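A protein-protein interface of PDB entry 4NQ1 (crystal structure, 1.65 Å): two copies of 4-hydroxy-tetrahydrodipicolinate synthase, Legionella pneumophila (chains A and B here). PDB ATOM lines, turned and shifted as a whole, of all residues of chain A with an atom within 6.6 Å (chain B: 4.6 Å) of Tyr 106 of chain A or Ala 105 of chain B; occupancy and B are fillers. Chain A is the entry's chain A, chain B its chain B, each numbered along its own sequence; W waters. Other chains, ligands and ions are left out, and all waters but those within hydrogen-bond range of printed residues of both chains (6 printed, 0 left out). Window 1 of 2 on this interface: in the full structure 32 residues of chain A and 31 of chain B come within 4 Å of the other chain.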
ATOM      1  N   GLY A  48      19.288  -6.527 -17.872  1.00  0.00           N
ATOM      2  CA  GLY A  48      19.387  -5.354 -18.799  1.00  0.00           C
ATOM      3  C   GLY A  48      20.711  -5.235 -19.565  1.00  0.00           C
ATOM      4  O   GLY A  48      20.744  -4.620 -20.607  1.00  0.00           O
ATOM      5  N   ASN A  79      11.456  -6.442 -25.231  1.00  0.00           N
ATOM      6  CA  ASN A  79      10.518  -5.413 -25.685  1.00  0.00           C
ATOM      7  C   ASN A  79       9.589  -5.820 -26.766  1.00  0.00           C
ATOM      8  O   ASN A  79       8.392  -5.634 -26.611  1.00  0.00           O
ATOM      9  CB  ASN A  79      11.299  -4.173 -26.192  1.00  0.00           C
ATOM     10  CG  ASN A  79      11.686  -3.246 -25.052  1.00  0.00           C
ATOM     11  OD1 ASN A  79      11.391  -3.495 -23.883  1.00  0.00           O
ATOM     12  ND2 ASN A  79      12.377  -2.175 -25.393  1.00  0.00           N
ATOM     13  N   PRO A 104       7.552  -4.200 -21.344  1.00  0.00           N
ATOM     14  CA  PRO A 104       8.507  -3.450 -22.228  1.00  0.00           C
ATOM     15  C   PRO A 104       8.974  -2.197 -21.496  1.00  0.00           C
ATOM     16  O   PRO A 104       8.217  -1.579 -20.711  1.00  0.00           O
ATOM     17  CB  PRO A 104       7.631  -3.057 -23.424  1.00  0.00           C
ATOM     18  CG  PRO A 104       6.559  -4.250 -23.433  1.00  0.00           C
ATOM     19  CD  PRO A 104       6.248  -4.500 -21.964  1.00  0.00           C
ATOM     20  N   ALA A 105      10.222  -1.857 -21.788  1.00  0.00           N
ATOM     21  CA  ALA A 105      10.768  -0.637 -21.242  1.00  0.00           C
ATOM     22  C   ALA A 105      11.019   0.370 -22.333  1.00  0.00           C
ATOM     23  O   ALA A 105      11.339   0.004 -23.457  1.00  0.00           O
ATOM     24  CB  ALA A 105      12.158  -1.019 -20.642  1.00  0.00           C
ATOM     25  N   TYR A 106      10.905   1.631 -21.925  1.00  0.00           N
ATOM     26  CA  TYR A 106      11.346   2.784 -22.737  1.00  0.00           C
ATOM     27  C   TYR A 106      10.387   3.134 -23.901  1.00  0.00           C
ATOM     28  O   TYR A 106      10.137   4.264 -24.178  1.00  0.00           O
ATOM     29  CB  TYR A 106      12.829   2.664 -23.156  1.00  0.00           C
ATOM     30  CG  TYR A 106      13.162   3.073 -24.564  1.00  0.00           C
ATOM     31  CD1 TYR A 106      13.098   4.386 -24.926  1.00  0.00           C
ATOM     32  CD2 TYR A 106      13.499   2.168 -25.500  1.00  0.00           C
ATOM     33  CE1 TYR A 106      13.413   4.793 -26.180  1.00  0.00           C
ATOM     34  CE2 TYR A 106      13.786   2.555 -26.786  1.00  0.00           C
ATOM     35  CZ  TYR A 106      13.745   3.865 -27.122  1.00  0.00           C
ATOM     36  OH  TYR A 106      13.999   4.344 -28.374  1.00  0.00           O
ATOM     37  N   ILE A 107       9.845   2.118 -24.531  1.00  0.00           N
ATOM     38  CA  ILE A 107       8.935   2.336 -25.719  1.00  0.00           C
ATOM     39  C   ILE A 107       7.503   2.700 -25.290  1.00  0.00           C
ATOM     40  O   ILE A 107       6.763   3.247 -26.088  1.00  0.00           O
ATOM     41  CB  ILE A 107       8.895   1.121 -26.664  1.00  0.00           C
ATOM     42  CG1 ILE A 107       8.394  -0.125 -25.935  1.00  0.00           C
ATOM     43  CG2 ILE A 107      10.340   0.830 -27.164  1.00  0.00           C
ATOM     44  CD1 ILE A 107       8.326  -1.338 -26.946  1.00  0.00           C
ATOM     45  N   LYS A 108       7.130   2.455 -24.034  1.00  0.00           N
ATOM     46  CA  LYS A 108       5.845   3.002 -23.515  1.00  0.00           C
ATOM     47  C   LYS A 108       4.551   2.589 -24.287  1.00  0.00           C
ATOM     48  O   LYS A 108       3.825   3.423 -24.788  1.00  0.00           O
ATOM     49  CB  LYS A 108       5.927   4.562 -23.303  1.00  0.00           C
ATOM     50  CG  LYS A 108       6.964   4.905 -22.198  1.00  0.00           C
ATOM     51  CD  LYS A 108       7.178   6.423 -22.088  1.00  0.00           C
ATOM     52  CE  LYS A 108       6.077   7.048 -21.463  1.00  0.00           C
ATOM     53  NZ  LYS A 108       6.570   8.458 -21.138  1.00  0.00           N
ATOM     54  N   PRO A 109       4.276   1.272 -24.284  1.00  0.00           N
ATOM     55  CA  PRO A 109       3.075   0.835 -24.999  1.00  0.00           C
ATOM     56  C   PRO A 109       1.836   1.310 -24.281  1.00  0.00           C
ATOM     57  O   PRO A 109       1.816   1.618 -23.081  1.00  0.00           O
ATOM     58  CB  PRO A 109       3.199  -0.725 -24.982  1.00  0.00           C
ATOM     59  CG  PRO A 109       4.074  -1.006 -23.796  1.00  0.00           C
ATOM     60  CD  PRO A 109       5.012   0.190 -23.595  1.00  0.00           C
ATOM     61  N   ARG A 137      11.298   2.124 -13.406  1.00  0.00           N
ATOM     62  CA  ARG A 137      12.420   1.839 -14.328  1.00  0.00           C
ATOM     63  C   ARG A 137      11.949   1.816 -15.782  1.00  0.00           C
ATOM     64  O   ARG A 137      12.742   2.167 -16.668  1.00  0.00           O
ATOM     65  CB  ARG A 137      13.020   0.430 -14.071  1.00  0.00           C
ATOM     66  CG  ARG A 137      13.746   0.317 -12.749  1.00  0.00           C
ATOM     67  CD  ARG A 137      14.197  -1.083 -12.551  1.00  0.00           C
ATOM     68  NE  ARG A 137      15.016  -1.325 -11.338  1.00  0.00           N
ATOM     69  CZ  ARG A 137      16.351  -1.360 -11.396  1.00  0.00           C
ATOM     70  NH1 ARG A 137      16.993  -1.109 -12.544  1.00  0.00           N
ATOM     71  NH2 ARG A 137      17.064  -1.625 -10.259  1.00  0.00           N
ATOM     72  N   THR A 138      10.721   1.359 -16.094  1.00  0.00           N
ATOM     73  CA  THR A 138      10.399   1.133 -17.502  1.00  0.00           C
ATOM     74  C   THR A 138       9.638   2.282 -18.156  1.00  0.00           C
ATOM     75  O   THR A 138       9.431   2.264 -19.393  1.00  0.00           O
ATOM     76  CB  THR A 138       9.420  -0.049 -17.635  1.00  0.00           C
ATOM     77  OG1 THR A 138       8.303   0.303 -16.834  1.00  0.00           O
ATOM     78  CG2 THR A 138      10.039  -1.342 -17.092  1.00  0.00           C
ATOM     79  N   ALA A 139       9.193   3.244 -17.340  1.00  0.00           N
ATOM     80  CA  ALA A 139       8.249   4.287 -17.766  1.00  0.00           C
ATOM     81  C   ALA A 139       6.881   3.765 -18.259  1.00  0.00           C
ATOM     82  O   ALA A 139       6.123   4.523 -18.876  1.00  0.00           O
ATOM     83  CB  ALA A 139       8.868   5.250 -18.817  1.00  0.00           C
ATOM     84  N   CYS A 140       6.570   2.502 -17.954  1.00  0.00           N
ATOM     85  CA  CYS A 140       5.273   1.851 -18.322  1.00  0.00           C
ATOM     86  C   CYS A 140       4.633   1.407 -17.008  1.00  0.00           C
ATOM     87  O   CYS A 140       5.207   0.637 -16.225  1.00  0.00           O
ATOM     88  CB  CYS A 140       5.595   0.686 -19.244  1.00  0.00           C
ATOM     89  SG  CYS A 140       4.078  -0.296 -19.513  1.00  0.00           S
ATOM     90  N   THR B  43      14.294   6.525 -31.741  1.00  0.00           N
ATOM     91  CA  THR B  43      13.110   6.073 -31.001  1.00  0.00           C
ATOM     92  C   THR B  43      11.892   6.133 -31.924  1.00  0.00           C
ATOM     93  O   THR B  43      11.001   5.222 -31.887  1.00  0.00           O
ATOM     94  CB  THR B  43      12.886   7.046 -29.815  1.00  0.00           C
ATOM     95  OG1 THR B  43      14.014   6.891 -28.953  1.00  0.00           O
ATOM     96  CG2 THR B  43      11.574   6.769 -29.034  1.00  0.00           C
ATOM     97  N   ALA B  47      13.503   1.744 -32.645  1.00  0.00           N
ATOM     98  CA  ALA B  47      14.712   1.109 -32.236  1.00  0.00           C
ATOM     99  C   ALA B  47      14.462   0.092 -31.097  1.00  0.00           C
ATOM    100  O   ALA B  47      15.122  -0.973 -31.076  1.00  0.00           O
ATOM    101  CB  ALA B  47      15.679   2.183 -31.689  1.00  0.00           C
ATOM    102  N   GLY B  48      13.491   0.429 -30.234  1.00  0.00           N
ATOM    103  CA  GLY B  48      13.241  -0.400 -29.061  1.00  0.00           C
ATOM    104  C   GLY B  48      12.735  -1.814 -29.393  1.00  0.00           C
ATOM    105  O   GLY B  48      12.752  -2.674 -28.536  1.00  0.00           O
ATOM    106  N   ASN B  79      22.165  -1.078 -24.141  1.00  0.00           N
ATOM    107  CA  ASN B  79      22.380  -0.894 -22.684  1.00  0.00           C
ATOM    108  C   ASN B  79      23.770  -1.191 -22.206  1.00  0.00           C
ATOM    109  O   ASN B  79      24.315  -0.406 -21.424  1.00  0.00           O
ATOM    110  CB  ASN B  79      21.432  -1.780 -21.864  1.00  0.00           C
ATOM    111  CG  ASN B  79      20.048  -1.194 -21.671  1.00  0.00           C
ATOM    112  OD1 ASN B  79      19.192  -1.872 -21.024  1.00  0.00           O
ATOM    113  ND2 ASN B  79      19.809   0.024 -22.089  1.00  0.00           N
ATOM    114  N   MET B 102      21.268   7.179 -27.225  1.00  0.00           N
ATOM    115  CA  MET B 102      20.443   7.316 -26.026  1.00  0.00           C
ATOM    116  C   MET B 102      21.143   6.726 -24.796  1.00  0.00           C
ATOM    117  O   MET B 102      21.900   5.723 -24.925  1.00  0.00           O
ATOM    118  CB  MET B 102      19.137   6.520 -26.299  1.00  0.00           C
ATOM    119  CG  MET B 102      18.019   6.867 -25.241  1.00  0.00           C
ATOM    120  SD  MET B 102      16.484   5.911 -25.555  1.00  0.00           S
ATOM    121  CE  MET B 102      16.990   4.269 -25.031  1.00  0.00           C
ATOM    122  N   THR B 103      20.855   7.268 -23.589  1.00  0.00           N
ATOM    123  CA  THR B 103      21.345   6.626 -22.382  1.00  0.00           C
ATOM    124  C   THR B 103      20.813   5.178 -22.333  1.00  0.00           C
ATOM    125  O   THR B 103      19.742   4.867 -22.915  1.00  0.00           O
ATOM    126  CB  THR B 103      20.959   7.376 -21.105  1.00  0.00           C
ATOM    127  OG1 THR B 103      19.539   7.248 -20.932  1.00  0.00           O
ATOM    128  CG2 THR B 103      21.411   8.852 -21.176  1.00  0.00           C
ATOM    129  N   PRO B 104      21.460   4.318 -21.530  1.00  0.00           N
ATOM    130  CA  PRO B 104      20.822   3.021 -21.138  1.00  0.00           C
ATOM    131  C   PRO B 104      19.450   3.288 -20.535  1.00  0.00           C
ATOM    132  O   PRO B 104      19.213   4.350 -19.905  1.00  0.00           O
ATOM    133  CB  PRO B 104      21.770   2.500 -20.022  1.00  0.00           C
ATOM    134  CG  PRO B 104      23.215   3.102 -20.512  1.00  0.00           C
ATOM    135  CD  PRO B 104      22.812   4.544 -21.003  1.00  0.00           C
ATOM    136  N   ALA B 105      18.532   2.327 -20.795  1.00  0.00           N
ATOM    137  CA  ALA B 105      17.188   2.423 -20.329  1.00  0.00           C
ATOM    138  C   ALA B 105      17.000   1.379 -19.267  1.00  0.00           C
ATOM    139  O   ALA B 105      17.582   0.272 -19.351  1.00  0.00           O
ATOM    140  CB  ALA B 105      16.180   2.143 -21.501  1.00  0.00           C
ATOM    141  N   TYR B 106      16.197   1.760 -18.297  1.00  0.00           N
ATOM    142  CA  TYR B 106      15.625   0.831 -17.324  1.00  0.00           C
ATOM    143  C   TYR B 106      16.604   0.388 -16.202  1.00  0.00           C
ATOM    144  O   TYR B 106      16.202   0.197 -15.115  1.00  0.00           O
ATOM    145  CB  TYR B 106      14.897  -0.353 -18.023  1.00  0.00           C
ATOM    146  CG  TYR B 106      15.156  -1.734 -17.445  1.00  0.00           C
ATOM    147  CD1 TYR B 106      14.692  -2.041 -16.211  1.00  0.00           C
ATOM    148  CD2 TYR B 106      15.893  -2.657 -18.101  1.00  0.00           C
ATOM    149  CE1 TYR B 106      14.891  -3.261 -15.648  1.00  0.00           C
ATOM    150  CE2 TYR B 106      16.146  -3.901 -17.521  1.00  0.00           C
ATOM    151  CZ  TYR B 106      15.638  -4.195 -16.284  1.00  0.00           C
ATOM    152  OH  TYR B 106      15.802  -5.380 -15.583  1.00  0.00           O
ATOM    153  N   ILE B 107      17.893   0.284 -16.528  1.00  0.00           N
ATOM    154  CA  ILE B 107      18.916  -0.169 -15.563  1.00  0.00           C
ATOM    155  C   ILE B 107      19.456   0.960 -14.665  1.00  0.00           C
ATOM    156  O   ILE B 107      20.038   0.689 -13.609  1.00  0.00           O
ATOM    157  CB  ILE B 107      20.074  -0.945 -16.266  1.00  0.00           C
ATOM    158  CG1 ILE B 107      20.828  -0.041 -17.266  1.00  0.00           C
ATOM    159  CG2 ILE B 107      19.567  -2.196 -16.976  1.00  0.00           C
ATOM    160  CD1 ILE B 107      22.130  -0.738 -17.869  1.00  0.00           C
ATOM    161  N   ARG B 137      11.477   8.403 -20.708  1.00  0.00           N
ATOM    162  CA  ARG B 137      11.378   7.020 -21.253  1.00  0.00           C
ATOM    163  C   ARG B 137      12.345   6.074 -20.550  1.00  0.00           C
ATOM    164  O   ARG B 137      12.024   4.904 -20.334  1.00  0.00           O
ATOM    165  CB  ARG B 137      11.717   6.962 -22.726  1.00  0.00           C
ATOM    166  CG  ARG B 137      10.591   7.638 -23.545  1.00  0.00           C
ATOM    167  CD  ARG B 137      10.989   7.561 -24.983  1.00  0.00           C
ATOM    168  NE  ARG B 137       9.948   8.039 -25.946  1.00  0.00           N
ATOM    169  CZ  ARG B 137       9.133   7.199 -26.615  1.00  0.00           C
ATOM    170  NH1 ARG B 137       9.184   5.847 -26.420  1.00  0.00           N
ATOM    171  NH2 ARG B 137       8.290   7.739 -27.564  1.00  0.00           N
ATOM    172  N   THR B 138      13.560   6.576 -20.237  1.00  0.00           N
ATOM    173  CA  THR B 138      14.587   5.655 -19.798  1.00  0.00           C
ATOM    174  C   THR B 138      14.770   5.498 -18.286  1.00  0.00           C
ATOM    175  O   THR B 138      15.518   4.604 -17.828  1.00  0.00           O
ATOM    176  CB  THR B 138      15.991   6.186 -20.199  1.00  0.00           C
ATOM    177  OG1 THR B 138      16.143   7.481 -19.620  1.00  0.00           O
ATOM    178  CG2 THR B 138      16.089   6.295 -21.765  1.00  0.00           C
HETATM  179  O   HOH W   1      13.105   2.359 -19.432  1.00  0.00           O
HETATM  180  O   HOH W   2      12.267   2.841 -29.886  1.00  0.00           O
HETATM  181  O   HOH W   3      19.829  -1.866 -12.643  1.00  0.00           O
HETATM  182  O   HOH W   4       7.880   4.256 -28.451  1.00  0.00           O
HETATM  183  O   HOH W   5      16.446   4.578 -28.706  1.00  0.00           O
HETATM  184  O   HOH W   6      18.574  -5.546 -15.340  1.00  0.00           O
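The side-chain amide oxygen (OD1) of Asn 79 of chain A is in hydrogen-bond range of the backbone NH (N) of Ala 105 of chain A. The backbone NH (N) of Tyr 106 of chain A is in hydrogen-bond range of the backbone carbonyl oxygen (O) of Thr 138 of chain A, at 3.0 Å. OG1 of Thr 138 of chain A lies within hydrogen-bond range of N of Cys 140 of chain A (3.0 Å). ND2 of Asn 79 of chain B lies close to N of Ala 105 of chain B (2.9 Å). The backbone NH of Tyr 106 of chain B sits at hydrogen-bond distance from the backbone carbonyl oxygen of Thr 138 of chain B, 3.0 Å away.
The backbone carbonyl oxygen (O) of Gly 48 of chain A lies close to the side-chain amide oxygen (OD1) of Asn 79 of chain B (3.2 Å). The backbone carbonyl oxygen (O) of Gly 48 of chain B sits close to the side-chain amide nitrogen (ND2) of Asn 79 of chain A, at 3.2 Å. OG1 of Thr 43 of chain B is in hydrogen-bond range of OH of Tyr 106 of chain A. The guanidinium group (NH1) of Arg 137 of chain B lies within hydrogen-bond range of the backbone carbonyl oxygen (O) of Tyr 106 of chain A (2.9 Å). The guanidinium group (NH1) of Arg 137 of chain A sits at hydrogen-bond distance from the backbone carbonyl oxygen (O) of Tyr 106 of chain B (3.0 Å).
Printed residues of chain A that touch a printed residue of chain B: Gly 48, Asn 79, Ala 105, Tyr 106, Ile 107, Lys 108, Arg 137, Thr 138 and Ala 139. Hydrophobic or aromatic side chains of chain A within 4 Å of the printed part of chain B: Ala 105, Tyr 106, Ile 107 and Ala 139. Along chain B the printed residues that touch a printed residue of chain A span positions 43 to 138. Among the printed residues, no Asp or Glu carboxylate lies within 4 Å of a Lys or Arg side-chain nitrogen of the other chain.
Gly 48 of chain A touches Ile 107 of chain B, and with the chains exchanged Ile 107 of chain A touches Gly 48 of chain B. Ala 105 of chain A touches Tyr 106 of chain B, and with the chains exchanged Tyr 106 of chain A touches Ala 105 of chain B. Ile 107 of chain A touches Arg 137 of chain B, and with the chains exchanged Arg 137 of chain A touches Ile 107 of chain B. Arg 137 of chain A touches Thr 138 of chain B, and with the chains exchanged Thr 138 of chain A touches Arg 137 of chain B. Of the 18 pairs that touch across the chains among the printed residues, 14 have their exchanged pair printed and touching as well.
Gly 48 of chain A touches Tyr 106 of chain B. Ile 107 of chain B touches Gly 48 of chain A (CG2 to CA, 3.7 Å). Ala 105 of chain A touches Tyr 106 of chain B (CB to CB, 3.8 Å). Tyr 106 of chain A touches Gly 48 of chain B. CE1 of Tyr 106 of chain A touches SD of Met 102 of chain B (3.3 Å). Tyr 106 of chain A touches Ala 105 of chain B. CG2 of Ile 107 of chain A touches CA of Gly 48 of chain B, at 3.7 Å. Ile 107 of chain A touches Arg 137 of chain B. CD of Lys 108 of chain A touches CG of Arg 137 of chain B, 3.9 Å away. Arg 137 of chain B touches Thr 138 of chain A (O to O, 3.8 Å).
Printed residues of chain B within 4 Å of Gly 48 of chain A: Asn 79 (3.2 Å), Tyr 106 (3.8 Å) and Ile 107 (3.7 Å). Printed residues of chain B within 4 Å of Ala 105 of chain A: Tyr 106 (3.8 Å). Of the printed residues of chain B, Thr 138 of chain A touches Arg 137 (3.8 Å). Of the printed residues of chain A, Met 102 of chain B touches Tyr 106 (3.3 Å). Printed residues of chain A within 4 Å of Ala 105 of chain B: Tyr 106. Of the printed residues of chain A, Tyr 106 of chain B touches Gly 48, Ala 105 and Arg 137.
Water W5 lies within hydrogen-bond range of OH of Tyr 106 of chain A (2.5 Å), OG1 of Thr 43 of chain B (3.4 Å) and SD of Met 102 of chain B (3.4 Å). Water W2 lies within hydrogen-bond range of the backbone NH of Gly 48 of chain B (2.7 Å), the side-chain hydroxyl of Tyr 106 of chain A (2.7 Å), the backbone NH of Ala 47 of chain B (3.2 Å) and the backbone carbonyl oxygen of Thr 43 of chain B (3.4 Å). Water W3 lies within hydrogen-bond range of O of Ile 107 of chain B (2.7 Å) and NH1 of Arg 137 of chain A (2.9 Å). Water W6 bridges the side-chain hydroxyl (OH) of Tyr 106 of chain B and the backbone NH (N) of Gly 48 of chain A. Water W1 lies within hydrogen-bond range of O of Arg 137 of chain A (2.8 Å), O of Arg 137 of chain B (2.9 Å), N of Tyr 106 of chain B (3.3 Å) and N of Tyr 106 of chain A (3.4 Å). Water W4 bridges O of Ile 107 of chain A (2.8 Å) and NH1 of Arg 137 of chain B (2.9 Å).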
